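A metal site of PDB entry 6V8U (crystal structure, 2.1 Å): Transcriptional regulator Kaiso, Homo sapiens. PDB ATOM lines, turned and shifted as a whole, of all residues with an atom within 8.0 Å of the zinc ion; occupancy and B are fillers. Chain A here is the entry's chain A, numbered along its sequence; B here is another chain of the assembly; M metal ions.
The backbone carbonyl oxygen (O) of Arg 31 is in hydrogen-bond range of the backbone NH (N) of Cys 26 (3.0 Å). The side-chain sulfur (SG) of Cys 29 sits close to the guanidinium group (NH1) of Arg 31 (3.1 Å). The side-chain hydroxyl (OH) of Tyr 33 lies close to a ring nitrogen (ND1) of His 42. SG of Cys 26 lies close to N of Val 28 (3.4 Å).
Of the 17 residues printed, 4 come within 4 Å of the zinc ion.
The zinc ion is bound by NE2 of His 46 (2.1 Å). The zinc ion is bound by NE2 of His 42. The side-chain sulfur (SG) of Cys 29 binds the zinc ion, at 2.2 Å. The side-chain sulfur (SG) of Cys 26 is bound to the zinc ion, at 2.3 Å. The zinc ion has four donor atoms within binding distance.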
ATOM      1  N   ASP A  12     -15.453 -10.481 -20.883  1.00  0.00           N
ATOM      2  CA  ASP A  12     -16.772 -10.233 -21.444  1.00  0.00           C
ATOM      3  C   ASP A  12     -17.846 -11.188 -20.925  1.00  0.00           C
ATOM      4  O   ASP A  12     -18.913 -11.283 -21.539  1.00  0.00           O
ATOM      5  CB  ASP A  12     -16.718 -10.305 -22.979  1.00  0.00           C
ATOM      6  CG  ASP A  12     -16.362 -11.686 -23.480  1.00  0.00           C
ATOM      7  OD1 ASP A  12     -15.725 -12.453 -22.715  1.00  0.00           O
ATOM      8  OD2 ASP A  12     -16.694 -12.009 -24.631  1.00  0.00           O
ATOM      9  N   ILE A  25     -22.236 -16.654 -19.129  1.00  0.00           N
ATOM     10  CA  ILE A  25     -23.204 -15.567 -19.050  1.00  0.00           C
ATOM     11  C   ILE A  25     -22.592 -14.325 -19.659  1.00  0.00           C
ATOM     12  O   ILE A  25     -21.527 -13.866 -19.207  1.00  0.00           O
ATOM     13  CB  ILE A  25     -23.636 -15.296 -17.598  1.00  0.00           C
ATOM     14  CG1 ILE A  25     -23.854 -16.604 -16.836  1.00  0.00           C
ATOM     15  CG2 ILE A  25     -24.864 -14.400 -17.582  1.00  0.00           C
ATOM     16  CD1 ILE A  25     -24.909 -17.505 -17.438  1.00  0.00           C
ATOM     17  N   CYS A  26     -23.255 -13.752 -20.646  1.00  0.00           N
ATOM     18  CA  CYS A  26     -22.807 -12.478 -21.198  1.00  0.00           C
ATOM     19  C   CYS A  26     -22.974 -11.373 -20.157  1.00  0.00           C
ATOM     20  O   CYS A  26     -24.020 -11.259 -19.509  1.00  0.00           O
ATOM     21  CB  CYS A  26     -23.620 -12.160 -22.441  1.00  0.00           C
ATOM     22  SG  CYS A  26     -23.377 -10.496 -23.012  1.00  0.00           S
ATOM     23  N   ILE A  27     -21.937 -10.532 -19.998  1.00  0.00           N
ATOM     24  CA  ILE A  27     -21.974  -9.506 -18.946  1.00  0.00           C
ATOM     25  C   ILE A  27     -22.978  -8.391 -19.247  1.00  0.00           C
ATOM     26  O   ILE A  27     -23.472  -7.743 -18.326  1.00  0.00           O
ATOM     27  CB  ILE A  27     -20.618  -8.826 -18.689  1.00  0.00           C
ATOM     28  CG1 ILE A  27     -19.864  -8.582 -19.996  1.00  0.00           C
ATOM     29  CG2 ILE A  27     -19.782  -9.603 -17.660  1.00  0.00           C
ATOM     30  CD1 ILE A  27     -18.616  -7.729 -19.822  1.00  0.00           C
ATOM     31  N   VAL A  28     -23.262  -8.137 -20.526  1.00  0.00           N
ATOM     32  CA  VAL A  28     -24.114  -7.003 -20.907  1.00  0.00           C
ATOM     33  C   VAL A  28     -25.590  -7.373 -20.754  1.00  0.00           C
ATOM     34  O   VAL A  28     -26.338  -6.689 -20.048  1.00  0.00           O
ATOM     35  CB  VAL A  28     -23.795  -6.567 -22.344  1.00  0.00           C
ATOM     36  CG1 VAL A  28     -24.884  -5.623 -22.882  1.00  0.00           C
ATOM     37  CG2 VAL A  28     -22.429  -5.916 -22.407  1.00  0.00           C
ATOM     38  N   CYS A  29     -26.020  -8.443 -21.427  1.00  0.00           N
ATOM     39  CA  CYS A  29     -27.433  -8.791 -21.451  1.00  0.00           C
ATOM     40  C   CYS A  29     -27.781 -10.007 -20.597  1.00  0.00           C
ATOM     41  O   CYS A  29     -28.971 -10.267 -20.395  1.00  0.00           O
ATOM     42  CB  CYS A  29     -27.907  -9.045 -22.902  1.00  0.00           C
ATOM     43  SG  CYS A  29     -27.128 -10.424 -23.768  1.00  0.00           S
ATOM     44  N   LYS A  30     -26.790 -10.732 -20.094  1.00  0.00           N
ATOM     45  CA  LYS A  30     -26.982 -11.894 -19.225  1.00  0.00           C
ATOM     46  C   LYS A  30     -27.624 -13.093 -19.928  1.00  0.00           C
ATOM     47  O   LYS A  30     -28.163 -13.978 -19.261  1.00  0.00           O
ATOM     48  CB  LYS A  30     -27.788 -11.513 -17.968  1.00  0.00           C
ATOM     49  CG  LYS A  30     -27.027 -10.592 -17.032  1.00  0.00           C
ATOM     50  CD  LYS A  30     -27.744  -9.264 -16.807  1.00  0.00           C
ATOM     51  CE  LYS A  30     -27.399  -8.684 -15.439  1.00  0.00           C
ATOM     52  NZ  LYS A  30     -28.432  -7.707 -14.970  1.00  0.00           N
ATOM     53  N   ARG A  31     -27.561 -13.158 -21.261  1.00  0.00           N
ATOM     54  CA  ARG A  31     -27.920 -14.401 -21.928  1.00  0.00           C
ATOM     55  C   ARG A  31     -26.913 -15.496 -21.558  1.00  0.00           C
ATOM     56  O   ARG A  31     -25.727 -15.220 -21.329  1.00  0.00           O
ATOM     57  CB  ARG A  31     -27.980 -14.211 -23.442  1.00  0.00           C
ATOM     58  CG  ARG A  31     -29.143 -13.316 -23.921  1.00  0.00           C
ATOM     59  CD  ARG A  31     -29.316 -13.354 -25.460  1.00  0.00           C
ATOM     60  NE  ARG A  31     -30.541 -12.673 -25.917  1.00  0.00           N
ATOM     61  CZ  ARG A  31     -30.708 -11.345 -25.886  1.00  0.00           C
ATOM     62  NH1 ARG A  31     -29.742 -10.557 -25.418  1.00  0.00           N
ATOM     63  NH2 ARG A  31     -31.842 -10.809 -26.309  1.00  0.00           N
ATOM     64  N   SER A  32     -27.387 -16.727 -21.448  1.00  0.00           N
ATOM     65  CA  SER A  32     -26.546 -17.858 -21.075  1.00  0.00           C
ATOM     66  C   SER A  32     -26.208 -18.719 -22.285  1.00  0.00           C
ATOM     67  O   SER A  32     -27.006 -18.883 -23.211  1.00  0.00           O
ATOM     68  CB  SER A  32     -27.196 -18.734 -20.012  1.00  0.00           C
ATOM     69  OG  SER A  32     -28.438 -19.243 -20.453  1.00  0.00           O
ATOM     70  N   TYR A  33     -25.022 -19.310 -22.250  1.00  0.00           N
ATOM     71  CA  TYR A  33     -24.522 -20.093 -23.367  1.00  0.00           C
ATOM     72  C   TYR A  33     -23.855 -21.341 -22.821  1.00  0.00           C
ATOM     73  O   TYR A  33     -23.069 -21.260 -21.865  1.00  0.00           O
ATOM     74  CB  TYR A  33     -23.533 -19.258 -24.204  1.00  0.00           C
ATOM     75  CG  TYR A  33     -24.263 -18.105 -24.864  1.00  0.00           C
ATOM     76  CD1 TYR A  33     -24.284 -16.847 -24.272  1.00  0.00           C
ATOM     77  CD2 TYR A  33     -24.984 -18.310 -26.036  1.00  0.00           C
ATOM     78  CE1 TYR A  33     -24.982 -15.804 -24.862  1.00  0.00           C
ATOM     79  CE2 TYR A  33     -25.691 -17.277 -26.630  1.00  0.00           C
ATOM     80  CZ  TYR A  33     -25.679 -16.026 -26.034  1.00  0.00           C
ATOM     81  OH  TYR A  33     -26.370 -14.989 -26.624  1.00  0.00           O
ATOM     82  N   LEU A  39     -20.981 -17.633 -26.911  1.00  0.00           N
ATOM     83  CA  LEU A  39     -20.980 -16.333 -26.262  1.00  0.00           C
ATOM     84  C   LEU A  39     -20.148 -15.324 -27.049  1.00  0.00           C
ATOM     85  O   LEU A  39     -20.548 -14.166 -27.180  1.00  0.00           O
ATOM     86  CB  LEU A  39     -20.466 -16.454 -24.818  1.00  0.00           C
ATOM     87  CG  LEU A  39     -20.619 -15.160 -24.018  1.00  0.00           C
ATOM     88  CD1 LEU A  39     -20.908 -15.475 -22.542  1.00  0.00           C
ATOM     89  CD2 LEU A  39     -19.375 -14.322 -24.131  1.00  0.00           C
ATOM     90  N   HIS A  42     -21.951 -14.230 -30.149  1.00  0.00           N
ATOM     91  CA  HIS A  42     -23.029 -13.344 -29.735  1.00  0.00           C
ATOM     92  C   HIS A  42     -22.509 -11.969 -29.308  1.00  0.00           C
ATOM     93  O   HIS A  42     -23.165 -10.945 -29.543  1.00  0.00           O
ATOM     94  CB  HIS A  42     -23.809 -13.980 -28.586  1.00  0.00           C
ATOM     95  CG  HIS A  42     -24.471 -12.976 -27.693  1.00  0.00           C
ATOM     96  ND1 HIS A  42     -25.686 -12.400 -27.977  1.00  0.00           N
ATOM     97  CD2 HIS A  42     -24.061 -12.437 -26.514  1.00  0.00           C
ATOM     98  CE1 HIS A  42     -26.004 -11.540 -27.022  1.00  0.00           C
ATOM     99  NE2 HIS A  42     -25.042 -11.556 -26.125  1.00  0.00           N
ATOM    100  N   PHE A  43     -21.356 -11.910 -28.639  1.00  0.00           N
ATOM    101  CA  PHE A  43     -20.939 -10.657 -28.024  1.00  0.00           C
ATOM    102  C   PHE A  43     -20.671  -9.574 -29.062  1.00  0.00           C
ATOM    103  O   PHE A  43     -20.782  -8.379 -28.741  1.00  0.00           O
ATOM    104  CB  PHE A  43     -19.692 -10.877 -27.159  1.00  0.00           C
ATOM    105  CG  PHE A  43     -19.445  -9.773 -26.144  1.00  0.00           C
ATOM    106  CD1 PHE A  43     -20.123  -9.768 -24.928  1.00  0.00           C
ATOM    107  CD2 PHE A  43     -18.552  -8.749 -26.408  1.00  0.00           C
ATOM    108  CE1 PHE A  43     -19.923  -8.756 -24.000  1.00  0.00           C
ATOM    109  CE2 PHE A  43     -18.330  -7.725 -25.479  1.00  0.00           C
ATOM    110  CZ  PHE A  43     -19.017  -7.731 -24.269  1.00  0.00           C
ATOM    111  N   ASN A  44     -20.332  -9.956 -30.290  1.00  0.00           N
ATOM    112  CA  ASN A  44     -20.124  -8.968 -31.335  1.00  0.00           C
ATOM    113  C   ASN A  44     -21.356  -8.087 -31.530  1.00  0.00           C
ATOM    114  O   ASN A  44     -21.227  -6.953 -32.004  1.00  0.00           O
ATOM    115  CB  ASN A  44     -19.745  -9.674 -32.629  1.00  0.00           C
ATOM    116  CG  ASN A  44     -18.959  -8.788 -33.558  1.00  0.00           C
ATOM    117  OD1 ASN A  44     -17.856  -8.327 -33.227  1.00  0.00           O
ATOM    118  ND2 ASN A  44     -19.505  -8.550 -34.750  1.00  0.00           N
ATOM    119  N   ILE A  45     -22.540  -8.574 -31.157  1.00  0.00           N
ATOM    120  CA  ILE A  45     -23.752  -7.753 -31.207  1.00  0.00           C
ATOM    121  C   ILE A  45     -23.618  -6.532 -30.287  1.00  0.00           C
ATOM    122  O   ILE A  45     -24.200  -5.476 -30.563  1.00  0.00           O
ATOM    123  CB  ILE A  45     -24.976  -8.605 -30.834  1.00  0.00           C
ATOM    124  CG1 ILE A  45     -25.194  -9.719 -31.875  1.00  0.00           C
ATOM    125  CG2 ILE A  45     -26.224  -7.755 -30.677  1.00  0.00           C
ATOM    126  CD1 ILE A  45     -26.279 -10.701 -31.475  1.00  0.00           C
ATOM    127  N   HIS A  46     -22.849  -6.657 -29.204  1.00  0.00           N
ATOM    128  CA  HIS A  46     -22.603  -5.535 -28.314  1.00  0.00           C
ATOM    129  C   HIS A  46     -21.381  -4.735 -28.735  1.00  0.00           C
ATOM    130  O   HIS A  46     -21.444  -3.499 -28.831  1.00  0.00           O
ATOM    131  CB  HIS A  46     -22.436  -6.028 -26.859  1.00  0.00           C
ATOM    132  CG  HIS A  46     -23.585  -6.835 -26.347  1.00  0.00           C
ATOM    133  ND1 HIS A  46     -24.888  -6.381 -26.371  1.00  0.00           N
ATOM    134  CD2 HIS A  46     -23.632  -8.062 -25.778  1.00  0.00           C
ATOM    135  CE1 HIS A  46     -25.684  -7.301 -25.852  1.00  0.00           C
ATOM    136  NE2 HIS A  46     -24.948  -8.324 -25.476  1.00  0.00           N
ATOM    137  P    DT B   8     -28.968 -16.809 -28.374  1.00  0.00           P
ATOM    138  OP1  DT B   8     -29.712 -16.793 -27.101  1.00  0.00           O
ATOM    139  OP2  DT B   8     -27.916 -15.790 -28.626  1.00  0.00           O
ATOM    140  O5'  DT B   8     -28.369 -18.259 -28.559  1.00  0.00           O
ATOM    141  C5'  DT B   8     -29.123 -19.370 -28.108  1.00  0.00           C
ATOM    142  C4'  DT B   8     -28.494 -20.659 -28.561  1.00  0.00           C
ATOM    143  O4'  DT B   8     -28.640 -20.782 -29.992  1.00  0.00           O
ATOM    144  C3'  DT B   8     -26.992 -20.811 -28.277  1.00  0.00           C
ATOM    145  O3'  DT B   8     -26.779 -22.169 -27.942  1.00  0.00           O
ATOM    146  C2'  DT B   8     -26.369 -20.473 -29.645  1.00  0.00           C
ATOM    147  C1'  DT B   8     -27.405 -21.128 -30.550  1.00  0.00           C
ATOM    148  N1   DT B   8     -27.426 -20.692 -31.982  1.00  0.00           N
ATOM    149  C2   DT B   8     -27.991 -21.556 -32.892  1.00  0.00           C
ATOM    150  O2   DT B   8     -28.436 -22.654 -32.595  1.00  0.00           O
ATOM    151  N3   DT B   8     -28.010 -21.121 -34.172  1.00  0.00           N
ATOM    152  C4   DT B   8     -27.541 -19.920 -34.652  1.00  0.00           C
ATOM    153  O4   DT B   8     -27.620 -19.632 -35.856  1.00  0.00           O
ATOM    154  C5   DT B   8     -26.961 -19.040 -33.664  1.00  0.00           C
ATOM    155  C7   DT B   8     -26.416 -17.708 -34.098  1.00  0.00           C
ATOM    156  C6   DT B   8     -26.934 -19.464 -32.379  1.00  0.00           C
HETATM  157 ZN    ZN M   1     -25.113 -10.159 -24.554  1.00  0.00          ZN
